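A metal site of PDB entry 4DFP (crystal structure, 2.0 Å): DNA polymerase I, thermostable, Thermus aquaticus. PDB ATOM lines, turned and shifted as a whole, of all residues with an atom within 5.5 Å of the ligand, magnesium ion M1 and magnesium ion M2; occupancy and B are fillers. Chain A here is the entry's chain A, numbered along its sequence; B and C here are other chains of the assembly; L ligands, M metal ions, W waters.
O12 of the ligand is in salt-bridge range of NH1 of Arg 367, at 2.6 Å. N4 of DOC 12 of chain C is in hydrogen-bond range of a nitrogen (N4) of the ligand, 3.4 Å away. N4 of the ligand lies within hydrogen-bond range of OG1 of Thr 372 (2.9 Å). N3 of DG 5 of chain B sits close to N2 of the ligand, 3.3 Å away. An oxygen (O2) of the ligand sits at hydrogen-bond distance from the backbone NH (N) of Glu 323 (3.0 Å). N of Gln 321 lies within hydrogen-bond range of O11 of the ligand (2.6 Å). NE2 of His 347 lies within hydrogen-bond range of O9 of the ligand. The guanidinium group (NH2) of Arg 281 is in hydrogen-bond range of an oxygen (O3) of the ligand, 3.2 Å away. O5 of the ligand is in salt-bridge range of NZ of Lys 371. A nitrogen (N2) of the ligand sits at hydrogen-bond distance from O2 of DC 4 of chain B.
Magnesium ion M2 is bound by water W6 (2.0 Å) and the side-chain carboxylate (OD2) of Asp 493 (2.2 Å). Slightly farther from magnesium ion M2 lies an oxygen (O6) of the ligand (2.6 Å).
Residues that only touch the ligand: Ile 322 (3.1 Å), Phe 375 (3.2 Å), Ser 320 (3.3 Å), Tyr 379 (3.3 Å) and Arg 368 (3.3 Å). Hydrophobic or aromatic side chains within 4 Å of the ligand: Ile 322, His 347, Phe 375 and Tyr 379.
Water W6 lies within hydrogen-bond range of the side-chain carboxylate of Glu 494 and the backbone carbonyl oxygen of Val 491. Water W2 lies within hydrogen-bond range of O5 of the ligand, OP2 of DOC 12 of chain C, NH1 of Arg 368 and NZ of Lys 371. Water W5 bridges an oxygen (O5) of the ligand and the side-chain amino group (NZ) of Lys 539. Water W3 lies within hydrogen-bond range of the side-chain carboxylate of Asp 318, an oxygen (O12) of the ligand and the side-chain amino group of Lys 371.
The side-chain carboxylate (OD2) of Asp 318 lies within salt-bridge range of the side-chain amino group (NZ) of Lys 539 (2.7 Å). O2 of DOC 12 of chain C lies within hydrogen-bond range of NH1 of Arg 281 (2.9 Å). OP2 of DOC 12 of chain C is in salt-bridge range of the guanidinium group of Arg 368 (2.4 Å). The side-chain amide nitrogen of Gln 321 is in hydrogen-bond range of the side-chain hydroxyl of Ser 320. N2 of DG 5 of chain B lies close to O2 of DOC 12 of chain C, 2.6 Å away. The side-chain hydroxyl of Tyr 379 sits at hydrogen-bond distance from the side-chain carboxylate of Glu 323 (2.6 Å). The guanidinium group of Arg 281 sits at hydrogen-bond distance from N2 of DG 5 of chain B.
Magnesium ion M1 is bound by OD1 of Asp 493 (2.0 Å), OD1 of Asp 318 (2.1 Å), O of Tyr 319 (2.1 Å), O6 of the ligand (2.2 Å), O8 of the ligand (2.2 Å) and O13 of the ligand (2.3 Å). Magnesium ion M1 has six donor atoms within binding distance.
Merely in contact with magnesium ion M2: DOC 12 of chain C (3.5 Å).
The nearest printed residue that does not touch magnesium ion M1 is Ser 320 (4.4 Å).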
ATOM      1  N   ARG A 281      14.577 -13.331  23.498  1.00  0.00           N
ATOM      2  CA  ARG A 281      13.825 -14.323  24.246  1.00  0.00           C
ATOM      3  C   ARG A 281      12.708 -13.637  25.020  1.00  0.00           C
ATOM      4  O   ARG A 281      12.762 -12.436  25.273  1.00  0.00           O
ATOM      5  CB  ARG A 281      14.733 -15.046  25.249  1.00  0.00           C
ATOM      6  CG  ARG A 281      15.293 -16.378  24.772  1.00  0.00           C
ATOM      7  CD  ARG A 281      15.947 -17.116  25.930  1.00  0.00           C
ATOM      8  NE  ARG A 281      16.436 -18.439  25.570  1.00  0.00           N
ATOM      9  CZ  ARG A 281      17.000 -19.271  26.435  1.00  0.00           C
ATOM     10  NH1 ARG A 281      17.142 -18.916  27.701  1.00  0.00           N
ATOM     11  NH2 ARG A 281      17.413 -20.470  26.034  1.00  0.00           N
ATOM     12  N   ASP A 318       9.047 -29.740  22.058  1.00  0.00           N
ATOM     13  CA  ASP A 318      10.386 -29.245  22.368  1.00  0.00           C
ATOM     14  C   ASP A 318      11.311 -29.395  21.164  1.00  0.00           C
ATOM     15  O   ASP A 318      11.554 -30.512  20.692  1.00  0.00           O
ATOM     16  CB  ASP A 318      10.948 -30.022  23.558  1.00  0.00           C
ATOM     17  CG  ASP A 318      12.122 -29.337  24.222  1.00  0.00           C
ATOM     18  OD1 ASP A 318      12.945 -28.729  23.498  1.00  0.00           O
ATOM     19  OD2 ASP A 318      12.225 -29.397  25.462  1.00  0.00           O
ATOM     20  N   TYR A 319      11.833 -28.271  20.661  1.00  0.00           N
ATOM     21  CA  TYR A 319      12.795 -28.311  19.561  1.00  0.00           C
ATOM     22  C   TYR A 319      14.022 -29.120  19.931  1.00  0.00           C
ATOM     23  O   TYR A 319      14.530 -29.030  21.055  1.00  0.00           O
ATOM     24  CB  TYR A 319      13.212 -26.900  19.133  1.00  0.00           C
ATOM     25  CG  TYR A 319      12.223 -26.177  18.228  1.00  0.00           C
ATOM     26  CD1 TYR A 319      12.157 -26.472  16.877  1.00  0.00           C
ATOM     27  CD2 TYR A 319      11.403 -25.172  18.719  1.00  0.00           C
ATOM     28  CE1 TYR A 319      11.268 -25.809  16.038  1.00  0.00           C
ATOM     29  CE2 TYR A 319      10.515 -24.503  17.893  1.00  0.00           C
ATOM     30  CZ  TYR A 319      10.456 -24.824  16.560  1.00  0.00           C
ATOM     31  OH  TYR A 319       9.575 -24.158  15.727  1.00  0.00           O
ATOM     32  N   SER A 320      14.494 -29.925  18.982  1.00  0.00           N
ATOM     33  CA  SER A 320      15.662 -30.770  19.193  1.00  0.00           C
ATOM     34  C   SER A 320      16.964 -30.003  18.978  1.00  0.00           C
ATOM     35  O   SER A 320      17.217 -29.518  17.875  1.00  0.00           O
ATOM     36  CB  SER A 320      15.616 -31.983  18.265  1.00  0.00           C
ATOM     37  OG  SER A 320      16.858 -32.681  18.291  1.00  0.00           O
ATOM     38  N   GLN A 321      17.773 -29.902  20.038  1.00  0.00           N
ATOM     39  CA  GLN A 321      19.111 -29.321  19.971  1.00  0.00           C
ATOM     40  C   GLN A 321      19.119 -27.988  19.226  1.00  0.00           C
ATOM     41  O   GLN A 321      19.977 -27.764  18.374  1.00  0.00           O
ATOM     42  CB  GLN A 321      20.071 -30.296  19.279  1.00  0.00           C
ATOM     43  CG  GLN A 321      19.923 -31.738  19.718  1.00  0.00           C
ATOM     44  CD  GLN A 321      20.719 -32.701  18.847  1.00  0.00           C
ATOM     45  OE1 GLN A 321      21.945 -32.664  18.832  1.00  0.00           O
ATOM     46  NE2 GLN A 321      20.009 -33.558  18.110  1.00  0.00           N
ATOM     47  N   ILE A 322      18.171 -27.128  19.557  1.00  0.00           N
ATOM     48  CA  ILE A 322      17.846 -25.983  18.693  1.00  0.00           C
ATOM     49  C   ILE A 322      19.001 -25.031  18.369  1.00  0.00           C
ATOM     50  O   ILE A 322      19.189 -24.681  17.206  1.00  0.00           O
ATOM     51  CB  ILE A 322      16.584 -25.211  19.185  1.00  0.00           C
ATOM     52  CG1 ILE A 322      16.098 -24.261  18.092  1.00  0.00           C
ATOM     53  CG2 ILE A 322      16.850 -24.463  20.479  1.00  0.00           C
ATOM     54  CD1 ILE A 322      15.755 -24.957  16.789  1.00  0.00           C
ATOM     55  N   GLU A 323      19.790 -24.650  19.370  1.00  0.00           N
ATOM     56  CA  GLU A 323      20.864 -23.686  19.122  1.00  0.00           C
ATOM     57  C   GLU A 323      22.018 -24.269  18.308  1.00  0.00           C
ATOM     58  O   GLU A 323      22.712 -23.545  17.597  1.00  0.00           O
ATOM     59  CB  GLU A 323      21.353 -23.053  20.436  1.00  0.00           C
ATOM     60  CG  GLU A 323      20.353 -22.078  21.030  1.00  0.00           C
ATOM     61  CD  GLU A 323      20.940 -21.227  22.149  1.00  0.00           C
ATOM     62  OE1 GLU A 323      22.175 -21.219  22.316  1.00  0.00           O
ATOM     63  OE2 GLU A 323      20.152 -20.565  22.857  1.00  0.00           O
ATOM     64  N   LEU A 324      22.219 -25.581  18.411  1.00  0.00           N
ATOM     65  CA  LEU A 324      23.243 -26.245  17.610  1.00  0.00           C
ATOM     66  C   LEU A 324      22.826 -26.281  16.139  1.00  0.00           C
ATOM     67  O   LEU A 324      23.660 -26.104  15.255  1.00  0.00           O
ATOM     68  CB  LEU A 324      23.510 -27.664  18.119  1.00  0.00           C
ATOM     69  CG  LEU A 324      24.144 -27.783  19.519  1.00  0.00           C
ATOM     70  CD1 LEU A 324      24.409 -29.240  19.866  1.00  0.00           C
ATOM     71  CD2 LEU A 324      25.435 -26.975  19.595  1.00  0.00           C
ATOM     72  N   HIS A 347      24.242 -34.062  22.013  1.00  0.00           N
ATOM     73  CA  HIS A 347      24.093 -34.156  23.464  1.00  0.00           C
ATOM     74  C   HIS A 347      24.302 -35.594  23.954  1.00  0.00           C
ATOM     75  O   HIS A 347      24.975 -35.821  24.958  1.00  0.00           O
ATOM     76  CB  HIS A 347      22.718 -33.649  23.894  1.00  0.00           C
ATOM     77  CG  HIS A 347      22.508 -32.194  23.644  1.00  0.00           C
ATOM     78  ND1 HIS A 347      23.548 -31.284  23.593  1.00  0.00           N
ATOM     79  CD2 HIS A 347      21.377 -31.474  23.423  1.00  0.00           C
ATOM     80  CE1 HIS A 347      23.066 -30.081  23.356  1.00  0.00           C
ATOM     81  NE2 HIS A 347      21.753 -30.174  23.239  1.00  0.00           N
ATOM     82  N   ARG A 367      22.311 -36.915  29.684  1.00  0.00           N
ATOM     83  CA  ARG A 367      22.197 -36.096  28.484  1.00  0.00           C
ATOM     84  C   ARG A 367      22.012 -34.622  28.851  1.00  0.00           C
ATOM     85  O   ARG A 367      22.544 -33.738  28.173  1.00  0.00           O
ATOM     86  CB  ARG A 367      21.022 -36.573  27.621  1.00  0.00           C
ATOM     87  CG  ARG A 367      20.909 -35.883  26.276  1.00  0.00           C
ATOM     88  CD  ARG A 367      19.794 -36.490  25.443  1.00  0.00           C
ATOM     89  NE  ARG A 367      19.676 -35.831  24.150  1.00  0.00           N
ATOM     90  CZ  ARG A 367      18.979 -34.713  23.934  1.00  0.00           C
ATOM     91  NH1 ARG A 367      18.338 -34.132  24.938  1.00  0.00           N
ATOM     92  NH2 ARG A 367      18.924 -34.185  22.718  1.00  0.00           N
ATOM     93  N   ARG A 368      21.269 -34.370  29.920  1.00  0.00           N
ATOM     94  CA  ARG A 368      21.051 -33.016  30.411  1.00  0.00           C
ATOM     95  C   ARG A 368      22.372 -32.363  30.808  1.00  0.00           C
ATOM     96  O   ARG A 368      22.622 -31.196  30.491  1.00  0.00           O
ATOM     97  CB  ARG A 368      20.106 -33.013  31.603  1.00  0.00           C
ATOM     98  CG  ARG A 368      19.952 -31.654  32.257  1.00  0.00           C
ATOM     99  CD  ARG A 368      19.121 -31.730  33.523  1.00  0.00           C
ATOM    100  NE  ARG A 368      18.920 -30.403  34.101  1.00  0.00           N
ATOM    101  CZ  ARG A 368      17.964 -29.557  33.728  1.00  0.00           C
ATOM    102  NH1 ARG A 368      17.121 -29.909  32.764  1.00  0.00           N
ATOM    103  NH2 ARG A 368      17.849 -28.373  34.309  1.00  0.00           N
ATOM    104  N   ALA A 369      23.214 -33.123  31.500  1.00  0.00           N
ATOM    105  CA  ALA A 369      24.524 -32.630  31.929  1.00  0.00           C
ATOM    106  C   ALA A 369      25.404 -32.298  30.727  1.00  0.00           C
ATOM    107  O   ALA A 369      26.230 -31.389  30.791  1.00  0.00           O
ATOM    108  CB  ALA A 369      25.202 -33.661  32.820  1.00  0.00           C
ATOM    109  N   LYS A 371      24.504 -30.953  28.029  1.00  0.00           N
ATOM    110  CA  LYS A 371      24.123 -29.657  27.482  1.00  0.00           C
ATOM    111  C   LYS A 371      24.991 -28.544  28.065  1.00  0.00           C
ATOM    112  O   LYS A 371      25.320 -27.575  27.372  1.00  0.00           O
ATOM    113  CB  LYS A 371      22.648 -29.357  27.761  1.00  0.00           C
ATOM    114  CG  LYS A 371      21.689 -30.329  27.099  1.00  0.00           C
ATOM    115  CD  LYS A 371      20.239 -29.976  27.423  1.00  0.00           C
ATOM    116  CE  LYS A 371      19.280 -30.944  26.744  1.00  0.00           C
ATOM    117  NZ  LYS A 371      17.856 -30.586  27.033  1.00  0.00           N
ATOM    118  N   THR A 372      25.363 -28.681  29.336  1.00  0.00           N
ATOM    119  CA  THR A 372      26.255 -27.739  29.977  1.00  0.00           C
ATOM    120  C   THR A 372      27.622 -27.759  29.289  1.00  0.00           C
ATOM    121  O   THR A 372      28.241 -26.716  29.077  1.00  0.00           O
ATOM    122  CB  THR A 372      26.453 -28.060  31.472  1.00  0.00           C
ATOM    123  OG1 THR A 372      25.197 -27.925  32.156  1.00  0.00           O
ATOM    124  CG2 THR A 372      27.465 -27.135  32.104  1.00  0.00           C
ATOM    125  N   PHE A 375      27.103 -26.555  25.134  1.00  0.00           N
ATOM    126  CA  PHE A 375      26.840 -25.128  24.993  1.00  0.00           C
ATOM    127  C   PHE A 375      27.869 -24.288  25.754  1.00  0.00           C
ATOM    128  O   PHE A 375      28.230 -23.198  25.316  1.00  0.00           O
ATOM    129  CB  PHE A 375      25.424 -24.777  25.440  1.00  0.00           C
ATOM    130  CG  PHE A 375      24.357 -25.404  24.588  1.00  0.00           C
ATOM    131  CD1 PHE A 375      24.245 -25.063  23.241  1.00  0.00           C
ATOM    132  CD2 PHE A 375      23.468 -26.326  25.114  1.00  0.00           C
ATOM    133  CE1 PHE A 375      23.267 -25.642  22.455  1.00  0.00           C
ATOM    134  CE2 PHE A 375      22.491 -26.896  24.324  1.00  0.00           C
ATOM    135  CZ  PHE A 375      22.394 -26.559  22.993  1.00  0.00           C
ATOM    136  N   GLY A 376      28.339 -24.806  26.884  1.00  0.00           N
ATOM    137  CA  GLY A 376      29.348 -24.130  27.671  1.00  0.00           C
ATOM    138  C   GLY A 376      30.621 -23.907  26.884  1.00  0.00           C
ATOM    139  O   GLY A 376      31.136 -22.788  26.816  1.00  0.00           O
ATOM    140  N   TYR A 379      30.225 -21.463  23.896  1.00  0.00           N
ATOM    141  CA  TYR A 379      30.107 -20.046  24.236  1.00  0.00           C
ATOM    142  C   TYR A 379      31.249 -19.531  25.108  1.00  0.00           C
ATOM    143  O   TYR A 379      31.132 -18.475  25.745  1.00  0.00           O
ATOM    144  CB  TYR A 379      28.740 -19.768  24.866  1.00  0.00           C
ATOM    145  CG  TYR A 379      27.603 -20.021  23.894  1.00  0.00           C
ATOM    146  CD1 TYR A 379      27.637 -19.489  22.616  1.00  0.00           C
ATOM    147  CD2 TYR A 379      26.507 -20.795  24.253  1.00  0.00           C
ATOM    148  CE1 TYR A 379      26.604 -19.712  21.717  1.00  0.00           C
ATOM    149  CE2 TYR A 379      25.481 -21.033  23.369  1.00  0.00           C
ATOM    150  CZ  TYR A 379      25.530 -20.487  22.099  1.00  0.00           C
ATOM    151  OH  TYR A 379      24.505 -20.708  21.206  1.00  0.00           O
ATOM    152  N   ASN A 458      26.878 -15.054  21.096  1.00  0.00           N
ATOM    153  CA  ASN A 458      25.791 -15.907  21.573  1.00  0.00           C
ATOM    154  C   ASN A 458      24.434 -15.398  21.112  1.00  0.00           C
ATOM    155  O   ASN A 458      23.543 -16.182  20.781  1.00  0.00           O
ATOM    156  CB  ASN A 458      25.809 -16.004  23.099  1.00  0.00           C
ATOM    157  CG  ASN A 458      24.558 -16.644  23.657  1.00  0.00           C
ATOM    158  OD1 ASN A 458      23.572 -15.965  23.946  1.00  0.00           O
ATOM    159  ND2 ASN A 458      24.577 -17.965  23.807  1.00  0.00           N
ATOM    160  N   VAL A 491       8.416 -22.086  27.047  1.00  0.00           N
ATOM    161  CA  VAL A 491       9.657 -22.146  27.808  1.00  0.00           C
ATOM    162  C   VAL A 491      10.836 -22.096  26.847  1.00  0.00           C
ATOM    163  O   VAL A 491      11.553 -23.081  26.671  1.00  0.00           O
ATOM    164  CB  VAL A 491       9.724 -23.402  28.707  1.00  0.00           C
ATOM    165  CG1 VAL A 491      10.865 -23.287  29.715  1.00  0.00           C
ATOM    166  CG2 VAL A 491       8.408 -23.604  29.442  1.00  0.00           C
ATOM    167  N   ASP A 493      12.233 -22.692  24.019  1.00  0.00           N
ATOM    168  CA  ASP A 493      12.104 -23.474  22.800  1.00  0.00           C
ATOM    169  C   ASP A 493      11.111 -24.616  22.972  1.00  0.00           C
ATOM    170  O   ASP A 493      11.105 -25.575  22.201  1.00  0.00           O
ATOM    171  CB  ASP A 493      13.470 -23.982  22.318  1.00  0.00           C
ATOM    172  CG  ASP A 493      13.918 -25.234  23.042  1.00  0.00           C
ATOM    173  OD1 ASP A 493      14.574 -26.067  22.387  1.00  0.00           O
ATOM    174  OD2 ASP A 493      13.640 -25.379  24.246  1.00  0.00           O
ATOM    175  N   GLU A 494      10.276 -24.482  23.992  1.00  0.00           N
ATOM    176  CA  GLU A 494       9.245 -25.465  24.275  1.00  0.00           C
ATOM    177  C   GLU A 494       7.887 -24.795  24.354  1.00  0.00           C
ATOM    178  O   GLU A 494       7.759 -23.675  24.863  1.00  0.00           O
ATOM    179  CB  GLU A 494       9.554 -26.169  25.597  1.00  0.00           C
ATOM    180  CG  GLU A 494       8.446 -27.073  26.107  1.00  0.00           C
ATOM    181  CD  GLU A 494       8.711 -27.575  27.514  1.00  0.00           C
ATOM    182  OE1 GLU A 494       9.753 -27.223  28.085  1.00  0.00           O
ATOM    183  OE2 GLU A 494       7.859 -28.319  28.051  1.00  0.00           O
ATOM    184  N   LYS A 539       6.605 -34.822  28.958  1.00  0.00           N
ATOM    185  CA  LYS A 539       7.934 -34.679  28.364  1.00  0.00           C
ATOM    186  C   LYS A 539       8.712 -35.989  28.396  1.00  0.00           C
ATOM    187  O   LYS A 539       9.890 -36.027  28.030  1.00  0.00           O
ATOM    188  CB  LYS A 539       8.728 -33.559  29.034  1.00  0.00           C
ATOM    189  CG  LYS A 539       8.175 -32.167  28.774  1.00  0.00           C
ATOM    190  CD  LYS A 539       9.247 -31.096  28.944  1.00  0.00           C
ATOM    191  CE  LYS A 539      10.292 -31.181  27.843  1.00  0.00           C
ATOM    192  NZ  LYS A 539      11.304 -30.100  27.935  1.00  0.00           N
ATOM    193  P    DC B   4      33.815 -19.635  32.677  1.00  0.00           P
ATOM    194  OP1  DC B   4      33.119 -19.745  33.971  1.00  0.00           O
ATOM    195  OP2  DC B   4      35.024 -20.457  32.420  1.00  0.00           O
ATOM    196  O5'  DC B   4      32.772 -19.938  31.497  1.00  0.00           O
ATOM    197  C5'  DC B   4      31.622 -19.120  31.374  1.00  0.00           C
ATOM    198  C4'  DC B   4      31.117 -19.096  29.937  1.00  0.00           C
ATOM    199  O4'  DC B   4      30.815 -20.446  29.511  1.00  0.00           O
ATOM    200  C3'  DC B   4      29.828 -18.314  29.753  1.00  0.00           C
ATOM    201  O3'  DC B   4      30.142 -16.960  29.442  1.00  0.00           O
ATOM    202  C2'  DC B   4      29.186 -19.021  28.560  1.00  0.00           C
ATOM    203  C1'  DC B   4      29.600 -20.469  28.785  1.00  0.00           C
ATOM    204  N1   DC B   4      28.622 -21.298  29.546  1.00  0.00           N
ATOM    205  C2   DC B   4      27.407 -21.679  28.953  1.00  0.00           C
ATOM    206  O2   DC B   4      27.177 -21.321  27.792  1.00  0.00           O
ATOM    207  N3   DC B   4      26.541 -22.435  29.660  1.00  0.00           N
ATOM    208  C4   DC B   4      26.832 -22.799  30.911  1.00  0.00           C
ATOM    209  N4   DC B   4      25.936 -23.544  31.569  1.00  0.00           N
ATOM    210  C5   DC B   4      28.048 -22.425  31.539  1.00  0.00           C
ATOM    211  C6   DC B   4      28.906 -21.680  30.830  1.00  0.00           C
ATOM    212  P    DG B   5      29.333 -15.772  30.154  1.00  0.00           P
ATOM    213  OP1  DG B   5      30.096 -14.521  29.973  1.00  0.00           O
ATOM    214  OP2  DG B   5      28.960 -16.216  31.518  1.00  0.00           O
ATOM    215  O5'  DG B   5      27.982 -15.674  29.300  1.00  0.00           O
ATOM    216  C5'  DG B   5      28.047 -15.293  27.930  1.00  0.00           C
ATOM    217  C4'  DG B   5      26.731 -15.588  27.229  1.00  0.00           C
ATOM    218  O4'  DG B   5      26.511 -17.021  27.213  1.00  0.00           O
ATOM    219  C3'  DG B   5      25.492 -15.009  27.904  1.00  0.00           C
ATOM    220  O3'  DG B   5      25.282 -13.675  27.475  1.00  0.00           O
ATOM    221  C2'  DG B   5      24.409 -15.943  27.397  1.00  0.00           C
ATOM    222  C1'  DG B   5      25.132 -17.284  27.330  1.00  0.00           C
ATOM    223  N9   DG B   5      24.874 -18.136  28.492  1.00  0.00           N
ATOM    224  C8   DG B   5      25.737 -18.423  29.517  1.00  0.00           C
ATOM    225  N7   DG B   5      25.220 -19.220  30.418  1.00  0.00           N
ATOM    226  C5   DG B   5      23.939 -19.469  29.950  1.00  0.00           C
ATOM    227  C6   DG B   5      22.901 -20.262  30.491  1.00  0.00           C
ATOM    228  O6   DG B   5      22.906 -20.940  31.536  1.00  0.00           O
ATOM    229  N1   DG B   5      21.755 -20.241  29.695  1.00  0.00           N
ATOM    230  C2   DG B   5      21.631 -19.531  28.520  1.00  0.00           C
ATOM    231  N2   DG B   5      20.447 -19.634  27.888  1.00  0.00           N
ATOM    232  N3   DG B   5      22.591 -18.783  27.996  1.00  0.00           N
ATOM    233  C4   DG B   5      23.714 -18.802  28.770  1.00  0.00           C
ATOM    234  N1  DOC C  12      17.552 -22.949  29.828  1.00  0.00           N
ATOM    235  C2  DOC C  12      18.588 -22.083  29.603  1.00  0.00           C
ATOM    236  N3  DOC C  12      19.734 -22.186  30.335  1.00  0.00           N
ATOM    237  C4  DOC C  12      19.895 -23.131  31.300  1.00  0.00           C
ATOM    238  C5  DOC C  12      18.845 -24.018  31.551  1.00  0.00           C
ATOM    239  C6  DOC C  12      17.655 -23.915  30.791  1.00  0.00           C
ATOM    240  O2  DOC C  12      18.508 -21.211  28.748  1.00  0.00           O
ATOM    241  N4  DOC C  12      21.113 -23.207  32.046  1.00  0.00           N
ATOM    242  C1' DOC C  12      16.319 -22.863  29.078  1.00  0.00           C
ATOM    243  C2' DOC C  12      16.323 -23.659  27.833  1.00  0.00           C
ATOM    244  C3' DOC C  12      15.420 -24.797  28.090  1.00  0.00           C
ATOM    245  C4' DOC C  12      14.477 -24.278  29.065  1.00  0.00           C
ATOM    246  O4' DOC C  12      15.222 -23.291  29.851  1.00  0.00           O
ATOM    247  C5' DOC C  12      14.025 -25.352  29.936  1.00  0.00           C
ATOM    248  O5' DOC C  12      15.013 -26.113  30.579  1.00  0.00           O
ATOM    249  P   DOC C  12      14.626 -27.029  31.763  1.00  0.00           P
ATOM    250  OP1 DOC C  12      13.344 -27.867  31.444  1.00  0.00           O
ATOM    251  OP2 DOC C  12      15.884 -27.906  32.106  1.00  0.00           O
HETATM  252  O1  LIG L   1      23.478 -24.515  29.850  1.00  0.00           O
HETATM  253  C1  LIG L   1      23.177 -23.838  28.841  1.00  0.00           C
HETATM  254  N1  LIG L   1      23.994 -22.867  28.399  1.00  0.00           N
HETATM  255  C2  LIG L   1      23.676 -22.129  27.303  1.00  0.00           C
HETATM  256  N2  LIG L   1      24.515 -21.165  26.871  1.00  0.00           N
HETATM  257  N3  LIG L   1      22.534 -22.354  26.621  1.00  0.00           N
HETATM  258  C3  LIG L   1      21.998 -24.088  28.149  1.00  0.00           C
HETATM  259  C4  LIG L   1      21.674 -23.317  27.031  1.00  0.00           C
HETATM  260  C5  LIG L   1      20.914 -24.928  28.258  1.00  0.00           C
HETATM  261  C6  LIG L   1      20.747 -25.882  29.188  1.00  0.00           C
HETATM  262  C7  LIG L   1      20.599 -26.726  30.000  1.00  0.00           C
HETATM  263  C8  LIG L   1      20.386 -27.818  30.963  1.00  0.00           C
HETATM  264  C9  LIG L   1      21.682 -28.214  31.680  1.00  0.00           C
HETATM  265  C10 LIG L   1      22.123 -27.133  32.670  1.00  0.00           C
HETATM  266  N4  LIG L   1      22.886 -26.107  31.977  1.00  0.00           N
HETATM  267  C11 LIG L   1      19.986 -24.733  27.270  1.00  0.00           C
HETATM  268  N5  LIG L   1      20.485 -23.716  26.544  1.00  0.00           N
HETATM  269  C12 LIG L   1      19.843 -23.155  25.331  1.00  0.00           C
HETATM  270  C13 LIG L   1      20.418 -23.938  24.164  1.00  0.00           C
HETATM  271  C14 LIG L   1      19.290 -24.858  23.739  1.00  0.00           C
HETATM  272  O2  LIG L   1      19.317 -25.032  22.321  1.00  0.00           O
HETATM  273  O3  LIG L   1      18.432 -23.391  25.361  1.00  0.00           O
HETATM  274  C15 LIG L   1      18.039 -24.122  24.199  1.00  0.00           C
HETATM  275  C16 LIG L   1      16.899 -25.068  24.536  1.00  0.00           C
HETATM  276  O4  LIG L   1      17.293 -25.861  25.659  1.00  0.00           O
HETATM  277  P1  LIG L   1      16.991 -27.437  25.687  1.00  0.00           P
HETATM  278  O5  LIG L   1      17.096 -27.901  27.127  1.00  0.00           O
HETATM  279  O6  LIG L   1      15.773 -27.794  24.875  1.00  0.00           O
HETATM  280  O7  LIG L   1      18.315 -27.948  24.946  1.00  0.00           O
HETATM  281  P2  LIG L   1      18.279 -28.500  23.435  1.00  0.00           P
HETATM  282  O8  LIG L   1      17.023 -28.016  22.745  1.00  0.00           O
HETATM  283  O9  LIG L   1      19.622 -28.177  22.830  1.00  0.00           O
HETATM  284  O10 LIG L   1      18.211 -30.081  23.735  1.00  0.00           O
HETATM  285  P3  LIG L   1      16.930 -30.991  23.378  1.00  0.00           P
HETATM  286  O11 LIG L   1      17.228 -31.530  22.008  1.00  0.00           O
HETATM  287  O12 LIG L   1      16.939 -32.024  24.485  1.00  0.00           O
HETATM  288  O13 LIG L   1      15.753 -30.045  23.447  1.00  0.00           O
HETATM  289 MG    MG M   1      14.815 -27.984  22.906  1.00  0.00          MG
HETATM  290 MG    MG M   2      13.546 -26.820  25.863  1.00  0.00          MG
HETATM  291  O   HOH W   1      22.290 -19.841  24.744  1.00  0.00           O
HETATM  292  O   HOH W   2      17.350 -28.558  29.824  1.00  0.00           O
HETATM  293  O   HOH W   3      14.632 -30.799  26.219  1.00  0.00           O
HETATM  294  O   HOH W   4      13.508 -31.649  22.237  1.00  0.00           O
HETATM  295  O   HOH W   5      14.458 -28.722  28.138  1.00  0.00           O
HETATM  296  O   HOH W   6      12.288 -25.935  27.186  1.00  0.00           O
